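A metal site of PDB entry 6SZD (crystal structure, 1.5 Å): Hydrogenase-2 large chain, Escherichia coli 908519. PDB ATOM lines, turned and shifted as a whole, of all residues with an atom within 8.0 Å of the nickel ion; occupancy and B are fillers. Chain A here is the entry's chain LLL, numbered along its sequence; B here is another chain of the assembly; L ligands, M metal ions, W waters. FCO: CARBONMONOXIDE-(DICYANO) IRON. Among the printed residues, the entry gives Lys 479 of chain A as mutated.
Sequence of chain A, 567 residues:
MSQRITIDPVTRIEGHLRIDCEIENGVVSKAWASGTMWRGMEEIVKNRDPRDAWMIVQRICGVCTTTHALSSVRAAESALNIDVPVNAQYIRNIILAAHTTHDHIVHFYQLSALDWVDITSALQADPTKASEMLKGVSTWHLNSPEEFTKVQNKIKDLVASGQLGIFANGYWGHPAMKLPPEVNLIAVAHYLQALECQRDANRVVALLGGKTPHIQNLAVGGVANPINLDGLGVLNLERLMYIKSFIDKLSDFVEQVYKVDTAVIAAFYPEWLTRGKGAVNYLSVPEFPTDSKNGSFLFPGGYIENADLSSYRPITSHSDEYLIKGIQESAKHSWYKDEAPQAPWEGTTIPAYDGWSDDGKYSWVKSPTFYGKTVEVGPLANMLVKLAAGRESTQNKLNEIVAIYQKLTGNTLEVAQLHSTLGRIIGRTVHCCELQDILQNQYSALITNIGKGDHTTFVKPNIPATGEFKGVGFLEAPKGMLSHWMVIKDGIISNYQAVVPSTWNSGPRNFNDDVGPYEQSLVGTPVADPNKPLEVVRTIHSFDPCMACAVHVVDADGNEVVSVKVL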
ATOM      1  N   GLU A  14       7.865  21.523  25.018  1.00  0.00           N
ATOM      2  CA  GLU A  14       7.574  21.111  23.636  1.00  0.00           C
ATOM      3  C   GLU A  14       6.109  20.685  23.545  1.00  0.00           C
ATOM      4  O   GLU A  14       5.690  19.790  24.324  1.00  0.00           O
ATOM      5  CB  GLU A  14       8.511  19.979  23.205  1.00  0.00           C
ATOM      6  CG  GLU A  14       8.419  19.650  21.717  1.00  0.00           C
ATOM      7  CD  GLU A  14       7.081  19.143  21.197  1.00  0.00           C
ATOM      8  OE1 GLU A  14       6.421  18.388  21.923  1.00  0.00           O
ATOM      9  OE2 GLU A  14       6.684  19.489  20.006  1.00  0.00           O
ATOM     10  N   GLN A  58      11.977   9.830  13.413  1.00  0.00           N
ATOM     11  CA  GLN A  58      12.793  10.913  14.009  1.00  0.00           C
ATOM     12  C   GLN A  58      11.887  12.142  14.169  1.00  0.00           C
ATOM     13  O   GLN A  58      12.064  12.922  15.097  1.00  0.00           O
ATOM     14  CB  GLN A  58      13.990  11.262  13.145  1.00  0.00           C
ATOM     15  CG  GLN A  58      14.907  12.247  13.865  1.00  0.00           C
ATOM     16  CD  GLN A  58      16.279  12.506  13.311  1.00  0.00           C
ATOM     17  OE1 GLN A  58      17.152  13.010  14.050  1.00  0.00           O
ATOM     18  NE2 GLN A  58      16.421  12.292  11.996  1.00  0.00           N
ATOM     19  N   ILE A  60       8.990  12.376  15.190  1.00  0.00           N
ATOM     20  CA  ILE A  60       8.174  12.437  16.425  1.00  0.00           C
ATOM     21  C   ILE A  60       8.508  13.731  17.149  1.00  0.00           C
ATOM     22  O   ILE A  60       7.545  14.380  17.688  1.00  0.00           O
ATOM     23  CB  ILE A  60       8.351  11.185  17.281  1.00  0.00           C
ATOM     24  CG1 ILE A  60       7.628  10.007  16.645  1.00  0.00           C
ATOM     25  CG2 ILE A  60       7.884  11.438  18.700  1.00  0.00           C
ATOM     26  CD1 ILE A  60       7.925   8.683  17.290  1.00  0.00           C
ATOM     27  N   CYS A  61       9.777  14.117  17.192  1.00  0.00           N
ATOM     28  CA  CYS A  61      10.142  15.319  17.948  1.00  0.00           C
ATOM     29  C   CYS A  61      11.415  15.960  17.383  1.00  0.00           C
ATOM     30  O   CYS A  61      12.405  15.245  17.166  1.00  0.00           O
ATOM     31  CB  CYS A  61      10.276  14.941  19.407  1.00  0.00           C
ATOM     32  SG  CYS A  61      10.594  16.343  20.518  1.00  0.00           S
ATOM     33  N   GLY A  62      11.387  17.294  17.309  1.00  0.00           N
ATOM     34  CA  GLY A  62      12.542  18.088  16.934  1.00  0.00           C
ATOM     35  C   GLY A  62      13.293  18.712  18.101  1.00  0.00           C
ATOM     36  O   GLY A  62      14.357  19.253  17.829  1.00  0.00           O
ATOM     37  N   VAL A  63      12.737  18.708  19.298  1.00  0.00           N
ATOM     38  CA  VAL A  63      13.505  19.129  20.492  1.00  0.00           C
ATOM     39  C   VAL A  63      14.451  17.957  20.816  1.00  0.00           C
ATOM     40  O   VAL A  63      15.684  18.129  20.787  1.00  0.00           O
ATOM     41  CB  VAL A  63      12.602  19.506  21.656  1.00  0.00           C
ATOM     42  CG1 VAL A  63      13.443  19.853  22.861  1.00  0.00           C
ATOM     43  CG2 VAL A  63      11.709  20.672  21.264  1.00  0.00           C
ATOM     44  N   CYS A  64      13.898  16.789  21.090  1.00  0.00           N
ATOM     45  CA  CYS A  64      14.717  15.557  21.244  1.00  0.00           C
ATOM     46  C   CYS A  64      14.948  14.940  19.873  1.00  0.00           C
ATOM     47  O   CYS A  64      14.830  13.707  19.681  1.00  0.00           O
ATOM     48  CB  CYS A  64      14.190  14.603  22.292  1.00  0.00           C
ATOM     49  SG  CYS A  64      12.551  13.948  21.903  1.00  0.00           S
ATOM     50  N   THR A  65      15.410  15.765  18.947  1.00  0.00           N
ATOM     51  CA  THR A  65      15.944  15.239  17.673  1.00  0.00           C
ATOM     52  C   THR A  65      17.098  14.265  18.013  1.00  0.00           C
ATOM     53  O   THR A  65      17.646  14.277  19.147  1.00  0.00           O
ATOM     54  CB  THR A  65      16.265  16.389  16.719  1.00  0.00           C
ATOM     55  OG1 THR A  65      16.550  15.806  15.443  1.00  0.00           O
ATOM     56  CG2 THR A  65      17.423  17.222  17.184  1.00  0.00           C
ATOM     57  N   THR A  67      16.966  11.267  18.936  1.00  0.00           N
ATOM     58  CA  THR A  67      16.669  10.173  19.865  1.00  0.00           C
ATOM     59  C   THR A  67      15.785   9.116  19.224  1.00  0.00           C
ATOM     60  O   THR A  67      16.064   7.894  19.375  1.00  0.00           O
ATOM     61  CB  THR A  67      16.033  10.699  21.175  1.00  0.00           C
ATOM     62  OG1 THR A  67      14.722  11.222  20.945  1.00  0.00           O
ATOM     63  CG2 THR A  67      16.927  11.713  21.849  1.00  0.00           C
ATOM     64  N   HIS A  68      14.732   9.529  18.538  1.00  0.00           N
ATOM     65  CA  HIS A  68      13.813   8.553  17.873  1.00  0.00           C
ATOM     66  C   HIS A  68      14.498   7.929  16.676  1.00  0.00           C
ATOM     67  O   HIS A  68      14.198   6.730  16.358  1.00  0.00           O
ATOM     68  CB  HIS A  68      12.503   9.265  17.492  1.00  0.00           C
ATOM     69  CG  HIS A  68      11.742   9.685  18.669  1.00  0.00           C
ATOM     70  ND1 HIS A  68      11.037   8.780  19.464  1.00  0.00           N
ATOM     71  CD2 HIS A  68      11.604  10.913  19.216  1.00  0.00           C
ATOM     72  CE1 HIS A  68      10.470   9.464  20.437  1.00  0.00           C
ATOM     73  NE2 HIS A  68      10.844  10.756  20.348  1.00  0.00           N
ATOM     74  N   HIS A  99      23.918  16.219  21.635  1.00  0.00           N
ATOM     75  CA  HIS A  99      22.516  16.646  21.527  1.00  0.00           C
ATOM     76  C   HIS A  99      21.961  16.856  22.944  1.00  0.00           C
ATOM     77  O   HIS A  99      21.292  17.882  23.193  1.00  0.00           O
ATOM     78  CB  HIS A  99      21.645  15.623  20.794  1.00  0.00           C
ATOM     79  CG  HIS A  99      20.240  16.035  20.963  1.00  0.00           C
ATOM     80  ND1 HIS A  99      19.734  17.057  20.230  1.00  0.00           N
ATOM     81  CD2 HIS A  99      19.344  15.741  21.934  1.00  0.00           C
ATOM     82  CE1 HIS A  99      18.522  17.302  20.678  1.00  0.00           C
ATOM     83  NE2 HIS A  99      18.258  16.533  21.747  1.00  0.00           N
ATOM     84  N   ASP A 103      20.198  19.999  24.834  1.00  0.00           N
ATOM     85  CA  ASP A 103      18.792  19.865  25.256  1.00  0.00           C
ATOM     86  C   ASP A 103      18.675  20.308  26.732  1.00  0.00           C
ATOM     87  O   ASP A 103      17.809  21.133  27.034  1.00  0.00           O
ATOM     88  CB  ASP A 103      18.456  18.386  25.008  1.00  0.00           C
ATOM     89  CG  ASP A 103      17.016  18.027  24.955  1.00  0.00           C
ATOM     90  OD1 ASP A 103      16.319  18.430  25.927  1.00  0.00           O
ATOM     91  OD2 ASP A 103      16.638  17.220  24.056  1.00  0.00           O
ATOM     92  N   ALA A 477      17.123   8.780  26.680  1.00  0.00           N
ATOM     93  CA  ALA A 477      16.941  10.090  26.039  1.00  0.00           C
ATOM     94  C   ALA A 477      17.047  11.176  27.095  1.00  0.00           C
ATOM     95  O   ALA A 477      17.028  10.918  28.315  1.00  0.00           O
ATOM     96  CB  ALA A 477      15.597  10.118  25.342  1.00  0.00           C
ATOM     97  N   PRO A 478      17.109  12.458  26.690  1.00  0.00           N
ATOM     98  CA  PRO A 478      17.217  13.546  27.652  1.00  0.00           C
ATOM     99  C   PRO A 478      16.060  13.587  28.653  1.00  0.00           C
ATOM    100  O   PRO A 478      16.264  13.957  29.788  1.00  0.00           O
ATOM    101  CB  PRO A 478      17.154  14.806  26.764  1.00  0.00           C
ATOM    102  CG  PRO A 478      17.785  14.330  25.464  1.00  0.00           C
ATOM    103  CD  PRO A 478      17.301  12.930  25.300  1.00  0.00           C
ATOM    104  N   LYS A 479      14.879  13.103  28.258  1.00  0.00           N
ATOM    105  CA  LYS A 479      13.693  13.078  29.139  1.00  0.00           C
ATOM    106  C   LYS A 479      13.508  11.712  29.807  1.00  0.00           C
ATOM    107  O   LYS A 479      12.616  11.619  30.620  1.00  0.00           O
ATOM    108  CB  LYS A 479      12.421  13.449  28.378  1.00  0.00           C
ATOM    109  CG  LYS A 479      12.069  14.910  28.440  1.00  0.00           C
ATOM    110  CD  LYS A 479      12.280  15.728  27.204  1.00  0.00           C
ATOM    111  CE  LYS A 479      13.718  16.097  26.913  1.00  0.00           C
ATOM    112  NZ  LYS A 479      13.826  17.494  26.411  1.00  0.00           N
ATOM    113  N   VAL A 500       7.462   6.471  25.008  1.00  0.00           N
ATOM    114  CA  VAL A 500       8.398   7.618  25.016  1.00  0.00           C
ATOM    115  C   VAL A 500       8.479   8.127  26.443  1.00  0.00           C
ATOM    116  O   VAL A 500       7.552   7.958  27.213  1.00  0.00           O
ATOM    117  CB  VAL A 500       7.933   8.657  23.985  1.00  0.00           C
ATOM    118  CG1 VAL A 500       8.906   9.795  23.790  1.00  0.00           C
ATOM    119  CG2 VAL A 500       7.686   7.964  22.641  1.00  0.00           C
ATOM    120  N   PRO A 501       9.605   8.727  26.903  1.00  0.00           N
ATOM    121  CA  PRO A 501       9.717   9.063  28.313  1.00  0.00           C
ATOM    122  C   PRO A 501       8.598   9.969  28.806  1.00  0.00           C
ATOM    123  O   PRO A 501       8.021   9.702  29.873  1.00  0.00           O
ATOM    124  CB  PRO A 501      11.126   9.674  28.455  1.00  0.00           C
ATOM    125  CG  PRO A 501      11.626   9.861  27.055  1.00  0.00           C
ATOM    126  CD  PRO A 501      10.891   8.846  26.192  1.00  0.00           C
ATOM    127  N   SER A 502       8.210  10.991  28.046  1.00  0.00           N
ATOM    128  CA  SER A 502       7.101  11.866  28.507  1.00  0.00           C
ATOM    129  C   SER A 502       5.773  11.095  28.492  1.00  0.00           C
ATOM    130  O   SER A 502       4.849  11.517  29.181  1.00  0.00           O
ATOM    131  CB  SER A 502       7.016  13.122  27.673  1.00  0.00           C
ATOM    132  OG  SER A 502       8.099  13.984  27.954  1.00  0.00           O
ATOM    133  N   ASP A 544      10.388  18.438  32.221  1.00  0.00           N
ATOM    134  CA  ASP A 544      10.777  18.741  30.818  1.00  0.00           C
ATOM    135  C   ASP A 544       9.756  18.097  29.866  1.00  0.00           C
ATOM    136  O   ASP A 544      10.086  17.256  29.024  1.00  0.00           O
ATOM    137  CB  ASP A 544      12.188  18.237  30.628  1.00  0.00           C
ATOM    138  CG  ASP A 544      12.879  18.618  29.355  1.00  0.00           C
ATOM    139  OD1 ASP A 544      12.308  19.404  28.570  1.00  0.00           O
ATOM    140  OD2 ASP A 544      14.031  18.096  29.179  1.00  0.00           O
ATOM    141  N   PRO A 545       8.466  18.464  29.962  1.00  0.00           N
ATOM    142  CA  PRO A 545       7.463  17.880  29.101  1.00  0.00           C
ATOM    143  C   PRO A 545       7.758  18.026  27.609  1.00  0.00           C
ATOM    144  O   PRO A 545       8.133  19.078  27.104  1.00  0.00           O
ATOM    145  CB  PRO A 545       6.164  18.609  29.431  1.00  0.00           C
ATOM    146  CG  PRO A 545       6.420  19.161  30.816  1.00  0.00           C
ATOM    147  CD  PRO A 545       7.883  19.501  30.849  1.00  0.00           C
ATOM    148  N   CYS A 546       7.524  16.916  26.911  1.00  0.00           N
ATOM    149  CA  CYS A 546       7.584  16.912  25.441  1.00  0.00           C
ATOM    150  C   CYS A 546       6.339  16.184  24.939  1.00  0.00           C
ATOM    151  O   CYS A 546       6.285  14.954  25.057  1.00  0.00           O
ATOM    152  CB  CYS A 546       8.829  16.226  24.960  1.00  0.00           C
ATOM    153  SG  CYS A 546       8.970  16.344  23.170  1.00  0.00           S
ATOM    154  N   MET A 547       5.355  16.931  24.449  1.00  0.00           N
ATOM    155  CA  MET A 547       4.051  16.287  24.125  1.00  0.00           C
ATOM    156  C   MET A 547       4.013  15.701  22.719  1.00  0.00           C
ATOM    157  O   MET A 547       3.204  14.773  22.502  1.00  0.00           O
ATOM    158  CB  MET A 547       2.903  17.268  24.351  1.00  0.00           C
ATOM    159  CG  MET A 547       2.891  17.815  25.767  1.00  0.00           C
ATOM    160  SD  MET A 547       3.131  16.648  27.109  1.00  0.00           S
ATOM    161  CE  MET A 547       1.641  15.665  26.911  1.00  0.00           C
ATOM    162  N   ALA A 548       4.839  16.179  21.791  1.00  0.00           N
ATOM    163  CA  ALA A 548       4.989  15.535  20.477  1.00  0.00           C
ATOM    164  C   ALA A 548       5.577  14.144  20.750  1.00  0.00           C
ATOM    165  O   ALA A 548       5.098  13.121  20.215  1.00  0.00           O
ATOM    166  CB  ALA A 548       5.895  16.343  19.593  1.00  0.00           C
ATOM    167  N   CYS A 549       6.550  14.082  21.660  1.00  0.00           N
ATOM    168  CA  CYS A 549       7.085  12.805  22.175  1.00  0.00           C
ATOM    169  C   CYS A 549       6.020  11.996  22.899  1.00  0.00           C
ATOM    170  O   CYS A 549       5.856  10.798  22.617  1.00  0.00           O
ATOM    171  CB  CYS A 549       8.237  13.026  23.142  1.00  0.00           C
ATOM    172  SG  CYS A 549       9.817  13.180  22.281  1.00  0.00           S
ATOM    173  N   ALA A 550       5.275  12.601  23.829  1.00  0.00           N
ATOM    174  CA  ALA A 550       4.402  11.801  24.712  1.00  0.00           C
ATOM    175  C   ALA A 550       3.324  11.100  23.863  1.00  0.00           C
ATOM    176  O   ALA A 550       2.995   9.975  24.176  1.00  0.00           O
ATOM    177  CB  ALA A 550       3.748  12.693  25.720  1.00  0.00           C
ATOM    178  N   CYS B  21       6.585  19.225  15.277  1.00  0.00           N
ATOM    179  CA  CYS B  21       7.486  18.452  16.139  1.00  0.00           C
ATOM    180  C   CYS B  21       8.406  19.412  16.918  1.00  0.00           C
ATOM    181  O   CYS B  21       9.182  18.945  17.747  1.00  0.00           O
ATOM    182  CB  CYS B  21       8.318  17.453  15.334  1.00  0.00           C
ATOM    183  SG  CYS B  21       9.725  18.198  14.447  1.00  0.00           S
ATOM    184  N   THR B  22       8.359  20.713  16.575  1.00  0.00           N
ATOM    185  CA  THR B  22       9.152  21.839  17.188  1.00  0.00           C
ATOM    186  C   THR B  22      10.534  21.946  16.518  1.00  0.00           C
ATOM    187  O   THR B  22      11.268  22.916  16.741  1.00  0.00           O
ATOM    188  CB  THR B  22       9.204  21.764  18.722  1.00  0.00           C
ATOM    189  OG1 THR B  22       7.831  21.595  19.132  1.00  0.00           O
ATOM    190  CG2 THR B  22       9.808  22.986  19.374  1.00  0.00           C
HETATM  191 FE   FCO L   1      11.573  13.028  23.705  1.00  0.00          FE
HETATM  192  C1  FCO L   1      10.480  12.862  25.177  1.00  0.00           C
HETATM  193  N1  FCO L   1       9.770  12.712  26.095  1.00  0.00           N
HETATM  194  C2  FCO L   1      13.090  13.236  24.754  1.00  0.00           C
HETATM  195  N2  FCO L   1      14.041  13.268  25.406  1.00  0.00           N
HETATM  196  C3  FCO L   1      12.013  11.305  23.567  1.00  0.00           C
HETATM  197  O3  FCO L   1      12.316  10.212  23.536  1.00  0.00           O
HETATM  198 NI    NI M   1      10.808  15.246  22.540  1.00  0.00          NI
HETATM  199  O   HOH W   1      12.121  16.972  24.063  1.00  0.00           O
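The nickel ion is bound by the side-chain sulfur of Cys 546 (2.2 Å), the side-chain sulfur of Cys 64 (2.3 Å), the side-chain sulfur of Cys 549 (2.3 Å) and the side-chain sulfur of Cys 61 (2.3 Å). Slightly farther from the nickel ion lies water W1 (2.7 Å).
SG of Cys 64 binds FE of the ligand, at 2.2 Å. SG of Cys 549 is bound to FE of the ligand, 2.3 Å away. N of Lys 479 sits at hydrogen-bond distance from N2 of the ligand, at 3.0 Å. N1 of the ligand lies within hydrogen-bond range of N of Ser 502 (3.0 Å). A nitrogen (N1) of the ligand sits at hydrogen-bond distance from the side-chain hydroxyl of Ser 502, at 2.8 Å.
Of the 27 residues printed, 4 come within 4 Å of the nickel ion. The nearest printed residue that does not touch the nickel ion is Val 63 (4.7 Å).
Water W1 lies within hydrogen-bond range of NZ of Lys 479 (2.9 Å) and N of Cys 64 (3.5 Å).
The side-chain sulfur (SG) of Cys 546 sits close to the side-chain carboxylate (OE1) of Glu 14 (3.5 Å). N of Cys 546 lies within hydrogen-bond range of OG of Ser 502 (3.2 Å). The backbone carbonyl oxygen of Cys 64 is in hydrogen-bond range of the side-chain hydroxyl of Thr 67, 2.8 Å away. The side-chain sulfur (SG) of Cys 549 sits close to a ring nitrogen (NE2) of His 68, at 3.3 Å. The side-chain sulfur (SG) of Cys 61 lies close to the backbone NH (N) of Val 63.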
